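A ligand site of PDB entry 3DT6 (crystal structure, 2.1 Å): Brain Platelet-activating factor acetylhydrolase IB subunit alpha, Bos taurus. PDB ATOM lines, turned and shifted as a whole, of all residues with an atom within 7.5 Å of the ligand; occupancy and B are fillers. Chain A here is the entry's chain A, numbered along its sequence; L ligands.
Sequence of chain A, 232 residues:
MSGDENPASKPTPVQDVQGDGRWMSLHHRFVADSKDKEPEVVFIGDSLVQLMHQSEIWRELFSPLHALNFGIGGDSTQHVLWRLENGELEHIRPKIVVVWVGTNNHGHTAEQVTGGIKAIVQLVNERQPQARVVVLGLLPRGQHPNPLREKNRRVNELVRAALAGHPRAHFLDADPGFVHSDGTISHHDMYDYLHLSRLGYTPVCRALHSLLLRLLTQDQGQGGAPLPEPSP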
ATOM      1  N   GLY A  45      24.020 -24.043  -1.548  1.00  0.00           N
ATOM      2  CA  GLY A  45      23.487 -22.716  -1.349  1.00  0.00           C
ATOM      3  C   GLY A  45      22.127 -22.790  -0.643  1.00  0.00           C
ATOM      4  O   GLY A  45      21.833 -23.747   0.070  1.00  0.00           O
ATOM      5  N   ASP A  46      21.321 -21.761  -0.854  1.00  0.00           N
ATOM      6  CA  ASP A  46      20.007 -21.688  -0.208  1.00  0.00           C
ATOM      7  C   ASP A  46      18.928 -22.326  -1.104  1.00  0.00           C
ATOM      8  O   ASP A  46      19.224 -23.157  -1.977  1.00  0.00           O
ATOM      9  CB  ASP A  46      19.676 -20.231   0.181  1.00  0.00           C
ATOM     10  CG  ASP A  46      19.790 -19.269  -0.986  1.00  0.00           C
ATOM     11  OD1 ASP A  46      19.553 -19.699  -2.131  1.00  0.00           O
ATOM     12  OD2 ASP A  46      20.108 -18.088  -0.771  1.00  0.00           O
ATOM     13  N   SER A  47      17.675 -21.926  -0.892  1.00  0.00           N
ATOM     14  CA  SER A  47      16.583 -22.485  -1.667  1.00  0.00           C
ATOM     15  C   SER A  47      16.736 -22.204  -3.173  1.00  0.00           C
ATOM     16  O   SER A  47      16.091 -23.081  -4.005  1.00  0.00           O
ATOM     17  CB  SER A  47      15.234 -21.923  -1.210  1.00  0.00           C
ATOM     18  OG  SER A  47      15.160 -20.479  -1.331  1.00  0.00           O
ATOM     19  N   LEU A  48      17.454 -21.189  -3.626  1.00  0.00           N
ATOM     20  CA  LEU A  48      17.646 -21.005  -5.070  1.00  0.00           C
ATOM     21  C   LEU A  48      18.339 -22.212  -5.689  1.00  0.00           C
ATOM     22  O   LEU A  48      17.989 -22.631  -6.772  1.00  0.00           O
ATOM     23  CB  LEU A  48      18.411 -19.728  -5.356  1.00  0.00           C
ATOM     24  CG  LEU A  48      17.637 -18.460  -5.045  1.00  0.00           C
ATOM     25  CD1 LEU A  48      18.530 -17.248  -5.143  1.00  0.00           C
ATOM     26  CD2 LEU A  48      16.394 -18.254  -5.952  1.00  0.00           C
ATOM     27  N   VAL A  49      19.298 -22.776  -4.957  1.00  0.00           N
ATOM     28  CA  VAL A  49      20.006 -24.022  -5.344  1.00  0.00           C
ATOM     29  C   VAL A  49      19.100 -25.256  -5.142  1.00  0.00           C
ATOM     30  O   VAL A  49      18.911 -26.044  -6.075  1.00  0.00           O
ATOM     31  CB  VAL A  49      21.307 -24.193  -4.557  1.00  0.00           C
ATOM     32  CG1 VAL A  49      22.008 -25.504  -4.955  1.00  0.00           C
ATOM     33  CG2 VAL A  49      22.228 -23.012  -4.792  1.00  0.00           C
ATOM     34  N   GLN A  50      18.550 -25.403  -3.939  1.00  0.00           N
ATOM     35  CA  GLN A  50      17.664 -26.500  -3.594  1.00  0.00           C
ATOM     36  C   GLN A  50      16.508 -26.719  -4.580  1.00  0.00           C
ATOM     37  O   GLN A  50      16.296 -27.837  -5.039  1.00  0.00           O
ATOM     38  CB  GLN A  50      17.096 -26.283  -2.193  1.00  0.00           C
ATOM     39  CG  GLN A  50      16.053 -27.328  -1.751  1.00  0.00           C
ATOM     40  CD  GLN A  50      15.430 -26.913  -0.404  1.00  0.00           C
ATOM     41  OE1 GLN A  50      14.926 -25.800  -0.275  1.00  0.00           O
ATOM     42  NE2 GLN A  50      15.488 -27.800   0.590  1.00  0.00           N
ATOM     43  N   LEU A  51      15.780 -25.645  -4.908  1.00  0.00           N
ATOM     44  CA  LEU A  51      14.575 -25.758  -5.722  1.00  0.00           C
ATOM     45  C   LEU A  51      14.934 -25.942  -7.221  1.00  0.00           C
ATOM     46  O   LEU A  51      14.059 -26.286  -8.043  1.00  0.00           O
ATOM     47  CB  LEU A  51      13.662 -24.547  -5.514  1.00  0.00           C
ATOM     48  CG  LEU A  51      13.110 -24.496  -4.080  1.00  0.00           C
ATOM     49  CD1 LEU A  51      12.210 -23.273  -3.858  1.00  0.00           C
ATOM     50  CD2 LEU A  51      12.340 -25.769  -3.807  1.00  0.00           C
ATOM     51  N   ILE A  72      19.808 -25.889   0.673  1.00  0.00           N
ATOM     52  CA  ILE A  72      18.841 -25.983   1.797  1.00  0.00           C
ATOM     53  C   ILE A  72      18.125 -24.632   1.964  1.00  0.00           C
ATOM     54  O   ILE A  72      18.770 -23.605   2.166  1.00  0.00           O
ATOM     55  CB  ILE A  72      19.525 -26.330   3.157  1.00  0.00           C
ATOM     56  CG1 ILE A  72      20.218 -27.708   3.121  1.00  0.00           C
ATOM     57  CG2 ILE A  72      18.501 -26.257   4.324  1.00  0.00           C
ATOM     58  CD1 ILE A  72      20.924 -28.091   4.484  1.00  0.00           C
ATOM     59  N   GLY A  73      16.786 -24.671   1.934  1.00  0.00           N
ATOM     60  CA  GLY A  73      16.013 -23.480   2.055  1.00  0.00           C
ATOM     61  C   GLY A  73      16.301 -22.775   3.394  1.00  0.00           C
ATOM     62  O   GLY A  73      16.389 -23.440   4.442  1.00  0.00           O
ATOM     63  N   GLY A  74      16.474 -21.469   3.327  1.00  0.00           N
ATOM     64  CA  GLY A  74      16.684 -20.620   4.531  1.00  0.00           C
ATOM     65  C   GLY A  74      18.122 -20.444   4.994  1.00  0.00           C
ATOM     66  O   GLY A  74      18.403 -19.642   5.890  1.00  0.00           O
ATOM     67  N   ASP A  75      19.047 -21.144   4.339  1.00  0.00           N
ATOM     68  CA  ASP A  75      20.463 -21.088   4.731  1.00  0.00           C
ATOM     69  C   ASP A  75      21.084 -19.698   4.475  1.00  0.00           C
ATOM     70  O   ASP A  75      20.784 -19.035   3.448  1.00  0.00           O
ATOM     71  CB  ASP A  75      21.282 -22.193   4.025  1.00  0.00           C
ATOM     72  CG  ASP A  75      21.495 -23.409   4.901  1.00  0.00           C
ATOM     73  OD1 ASP A  75      20.734 -23.639   5.869  1.00  0.00           O
ATOM     74  OD2 ASP A  75      22.448 -24.148   4.610  1.00  0.00           O
ATOM     75  N   SER A  76      21.962 -19.274   5.404  1.00  0.00           N
ATOM     76  CA  SER A  76      22.756 -18.075   5.265  1.00  0.00           C
ATOM     77  C   SER A  76      24.208 -18.525   4.947  1.00  0.00           C
ATOM     78  O   SER A  76      24.489 -19.710   4.966  1.00  0.00           O
ATOM     79  CB  SER A  76      22.736 -17.230   6.562  1.00  0.00           C
ATOM     80  OG  SER A  76      21.512 -16.562   6.772  1.00  0.00           O
ATOM     81  N   THR A 103      21.359 -14.128   0.262  1.00  0.00           N
ATOM     82  CA  THR A 103      20.148 -13.306   0.291  1.00  0.00           C
ATOM     83  C   THR A 103      19.384 -13.471   1.625  1.00  0.00           C
ATOM     84  O   THR A 103      18.550 -12.655   1.978  1.00  0.00           O
ATOM     85  CB  THR A 103      19.239 -13.593  -0.926  1.00  0.00           C
ATOM     86  OG1 THR A 103      18.261 -12.543  -1.045  1.00  0.00           O
ATOM     87  CG2 THR A 103      18.492 -14.942  -0.779  1.00  0.00           C
ATOM     88  N   ASN A 104      19.686 -14.534   2.350  1.00  0.00           N
ATOM     89  CA  ASN A 104      19.029 -14.806   3.647  1.00  0.00           C
ATOM     90  C   ASN A 104      19.749 -14.269   4.881  1.00  0.00           C
ATOM     91  O   ASN A 104      19.289 -14.479   6.006  1.00  0.00           O
ATOM     92  CB  ASN A 104      18.810 -16.327   3.808  1.00  0.00           C
ATOM     93  CG  ASN A 104      17.812 -16.883   2.798  1.00  0.00           C
ATOM     94  OD1 ASN A 104      16.894 -16.194   2.358  1.00  0.00           O
ATOM     95  ND2 ASN A 104      17.975 -18.142   2.447  1.00  0.00           N
ATOM     96  N   LEU A 139      20.088 -12.399  -6.208  1.00  0.00           N
ATOM     97  CA  LEU A 139      19.007 -11.886  -7.050  1.00  0.00           C
ATOM     98  C   LEU A 139      18.226 -10.751  -6.367  1.00  0.00           C
ATOM     99  O   LEU A 139      18.173 -10.628  -5.147  1.00  0.00           O
ATOM    100  CB  LEU A 139      18.081 -13.018  -7.518  1.00  0.00           C
ATOM    101  CG  LEU A 139      18.623 -14.127  -8.393  1.00  0.00           C
ATOM    102  CD1 LEU A 139      17.499 -15.132  -8.657  1.00  0.00           C
ATOM    103  CD2 LEU A 139      19.201 -13.535  -9.708  1.00  0.00           C
ATOM    104  N   ARG A 141      14.806  -8.871  -5.115  1.00  0.00           N
ATOM    105  CA  ARG A 141      13.654  -9.496  -4.439  1.00  0.00           C
ATOM    106  C   ARG A 141      12.709  -8.361  -4.040  1.00  0.00           C
ATOM    107  O   ARG A 141      13.097  -7.195  -4.082  1.00  0.00           O
ATOM    108  CB  ARG A 141      14.103 -10.296  -3.193  1.00  0.00           C
ATOM    109  CG  ARG A 141      15.042  -9.451  -2.269  1.00  0.00           C
ATOM    110  CD  ARG A 141      15.597 -10.329  -1.130  1.00  0.00           C
ATOM    111  NE  ARG A 141      14.567 -10.637  -0.148  1.00  0.00           N
ATOM    112  CZ  ARG A 141      14.674 -11.554   0.804  1.00  0.00           C
ATOM    113  NH1 ARG A 141      15.771 -12.295   0.895  1.00  0.00           N
ATOM    114  NH2 ARG A 141      13.659 -11.750   1.671  1.00  0.00           N
ATOM    115  N   TYR A 191       7.137 -16.055  -7.951  1.00  0.00           N
ATOM    116  CA  TYR A 191       5.759 -16.132  -7.489  1.00  0.00           C
ATOM    117  C   TYR A 191       5.508 -15.398  -6.159  1.00  0.00           C
ATOM    118  O   TYR A 191       4.430 -14.869  -5.932  1.00  0.00           O
ATOM    119  CB  TYR A 191       5.271 -17.618  -7.439  1.00  0.00           C
ATOM    120  CG  TYR A 191       6.140 -18.527  -6.598  1.00  0.00           C
ATOM    121  CD1 TYR A 191       5.949 -18.627  -5.206  1.00  0.00           C
ATOM    122  CD2 TYR A 191       7.113 -19.341  -7.183  1.00  0.00           C
ATOM    123  CE1 TYR A 191       6.764 -19.485  -4.413  1.00  0.00           C
ATOM    124  CE2 TYR A 191       7.878 -20.191  -6.429  1.00  0.00           C
ATOM    125  CZ  TYR A 191       7.708 -20.262  -5.046  1.00  0.00           C
ATOM    126  OH  TYR A 191       8.487 -21.134  -4.306  1.00  0.00           O
ATOM    127  N   ASP A 192       6.529 -15.296  -5.314  1.00  0.00           N
ATOM    128  CA  ASP A 192       6.410 -14.569  -4.086  1.00  0.00           C
ATOM    129  C   ASP A 192       7.441 -13.452  -3.994  1.00  0.00           C
ATOM    130  O   ASP A 192       7.777 -12.960  -2.888  1.00  0.00           O
ATOM    131  CB  ASP A 192       6.527 -15.536  -2.895  1.00  0.00           C
ATOM    132  CG  ASP A 192       7.879 -16.250  -2.869  1.00  0.00           C
ATOM    133  OD1 ASP A 192       8.700 -16.020  -3.759  1.00  0.00           O
ATOM    134  OD2 ASP A 192       8.105 -17.045  -1.944  1.00  0.00           O
ATOM    135  N   LEU A 194      10.538 -13.613  -4.455  1.00  0.00           N
ATOM    136  CA  LEU A 194      11.789 -14.110  -3.871  1.00  0.00           C
ATOM    137  C   LEU A 194      12.250 -15.383  -4.547  1.00  0.00           C
ATOM    138  O   LEU A 194      13.383 -15.455  -5.112  1.00  0.00           O
ATOM    139  CB  LEU A 194      11.650 -14.325  -2.331  1.00  0.00           C
ATOM    140  CG  LEU A 194      12.869 -14.950  -1.598  1.00  0.00           C
ATOM    141  CD1 LEU A 194      14.101 -14.021  -1.783  1.00  0.00           C
ATOM    142  CD2 LEU A 194      12.539 -15.076  -0.121  1.00  0.00           C
ATOM    143  N   HIS A 195      11.366 -16.379  -4.557  1.00  0.00           N
ATOM    144  CA  HIS A 195      11.619 -17.679  -5.190  1.00  0.00           C
ATOM    145  C   HIS A 195      11.269 -17.628  -6.664  1.00  0.00           C
ATOM    146  O   HIS A 195      10.271 -17.044  -7.047  1.00  0.00           O
ATOM    147  CB  HIS A 195      10.805 -18.806  -4.538  1.00  0.00           C
ATOM    148  CG  HIS A 195      11.087 -18.972  -3.073  1.00  0.00           C
ATOM    149  ND1 HIS A 195      10.286 -18.424  -2.095  1.00  0.00           N
ATOM    150  CD2 HIS A 195      12.075 -19.615  -2.421  1.00  0.00           C
ATOM    151  CE1 HIS A 195      10.758 -18.735  -0.903  1.00  0.00           C
ATOM    152  NE2 HIS A 195      11.853 -19.445  -1.077  1.00  0.00           N
ATOM    153  N   LEU A 196      12.088 -18.297  -7.472  1.00  0.00           N
ATOM    154  CA  LEU A 196      11.902 -18.329  -8.926  1.00  0.00           C
ATOM    155  C   LEU A 196      10.841 -19.361  -9.348  1.00  0.00           C
ATOM    156  O   LEU A 196      10.799 -20.457  -8.820  1.00  0.00           O
ATOM    157  CB  LEU A 196      13.240 -18.707  -9.574  1.00  0.00           C
ATOM    158  CG  LEU A 196      14.311 -17.619  -9.453  1.00  0.00           C
ATOM    159  CD1 LEU A 196      15.630 -18.241  -9.795  1.00  0.00           C
ATOM    160  CD2 LEU A 196      13.945 -16.399 -10.356  1.00  0.00           C
ATOM    161  N   TYR A 201      13.433 -19.533 -13.590  1.00  0.00           N
ATOM    162  CA  TYR A 201      14.596 -20.406 -13.550  1.00  0.00           C
ATOM    163  C   TYR A 201      15.250 -20.638 -14.937  1.00  0.00           C
ATOM    164  O   TYR A 201      16.474 -20.857 -15.017  1.00  0.00           O
ATOM    165  CB  TYR A 201      14.220 -21.770 -12.948  1.00  0.00           C
ATOM    166  CG  TYR A 201      14.520 -21.929 -11.456  1.00  0.00           C
ATOM    167  CD1 TYR A 201      15.823 -21.757 -10.974  1.00  0.00           C
ATOM    168  CD2 TYR A 201      13.497 -22.274 -10.548  1.00  0.00           C
ATOM    169  CE1 TYR A 201      16.103 -21.916  -9.603  1.00  0.00           C
ATOM    170  CE2 TYR A 201      13.787 -22.430  -9.180  1.00  0.00           C
ATOM    171  CZ  TYR A 201      15.106 -22.242  -8.733  1.00  0.00           C
ATOM    172  OH  TYR A 201      15.406 -22.393  -7.392  1.00  0.00           O
HETATM  173  C1  LIG L   1      13.794 -20.872   2.004  1.00  0.00           C
HETATM  174  C2  LIG L   1      12.817 -22.059   2.197  1.00  0.00           C
HETATM  175  C3  LIG L   1      16.138 -17.612  -1.005  1.00  0.00           C
HETATM  176  C4  LIG L   1      15.678 -17.236  -2.391  1.00  0.00           C
HETATM  177  O1  LIG L   1      13.708 -20.115   0.752  1.00  0.00           O
HETATM  178  O2  LIG L   1      15.040 -18.094  -0.207  1.00  0.00           O
HETATM  179  O3  LIG L   1      16.300 -20.099   0.984  1.00  0.00           O
HETATM  180  P1  LIG L   1      15.083 -19.697   0.100  1.00  0.00           P
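A phosphorus (P1) of the ligand is bonded to the side-chain hydroxyl (OG) of Ser 47 (1.6 Å). The backbone NH (N) of Ser 47 is in hydrogen-bond range of an oxygen (O3) of the ligand (3.0 Å). The backbone NH (N) of Gly 74 lies within hydrogen-bond range of an oxygen (O3) of the ligand (2.7 Å). O1 of the ligand lies within hydrogen-bond range of NE2 of His 195 (2.7 Å). An oxygen (O3) of the ligand sits at hydrogen-bond distance from the side-chain amide nitrogen (ND2) of Asn 104, 3.0 Å away.
O of Leu 48 sits at hydrogen-bond distance from OH of Tyr 201, at 2.7 Å. The side-chain carboxylate (OD1) of Asp 46 lies within hydrogen-bond range of the backbone NH (N) of Leu 48, 3.0 Å away. OG of Ser 47 sits close to NE2 of His 195 (3.5 Å). A ring nitrogen (ND1) of His 195 lies within hydrogen-bond range of the side-chain carboxylate (OD2) of Asp 192 (2.6 Å). N of Leu 194 is in hydrogen-bond range of OD1 of Asp 192, at 3.1 Å. The backbone NH (N) of Gly 73 is in hydrogen-bond range of the side-chain amide oxygen (OE1) of Gln 50, 3.1 Å away. The backbone carbonyl oxygen (O) of Asn 104 is in hydrogen-bond range of the side-chain hydroxyl (OG) of Ser 76 (3.1 Å). NH1 of Arg 141 is in hydrogen-bond range of O of Thr 103 (3.0 Å).
Merely in contact with the ligand: Gly 73 (3.4 Å), Asp 46 (3.5 Å), Leu 48 (3.5 Å), Thr 103 (3.6 Å) and Leu 194 (3.6 Å). Hydrophobic or aromatic side chains that line the ligand: Leu 48, Leu 194 and His 195. Within 4 Å of the ligand: Asp 46, Ser 47, Leu 48, Gly 73, Gly 74, Thr 103, Asn 104, Leu 194 and His 195.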
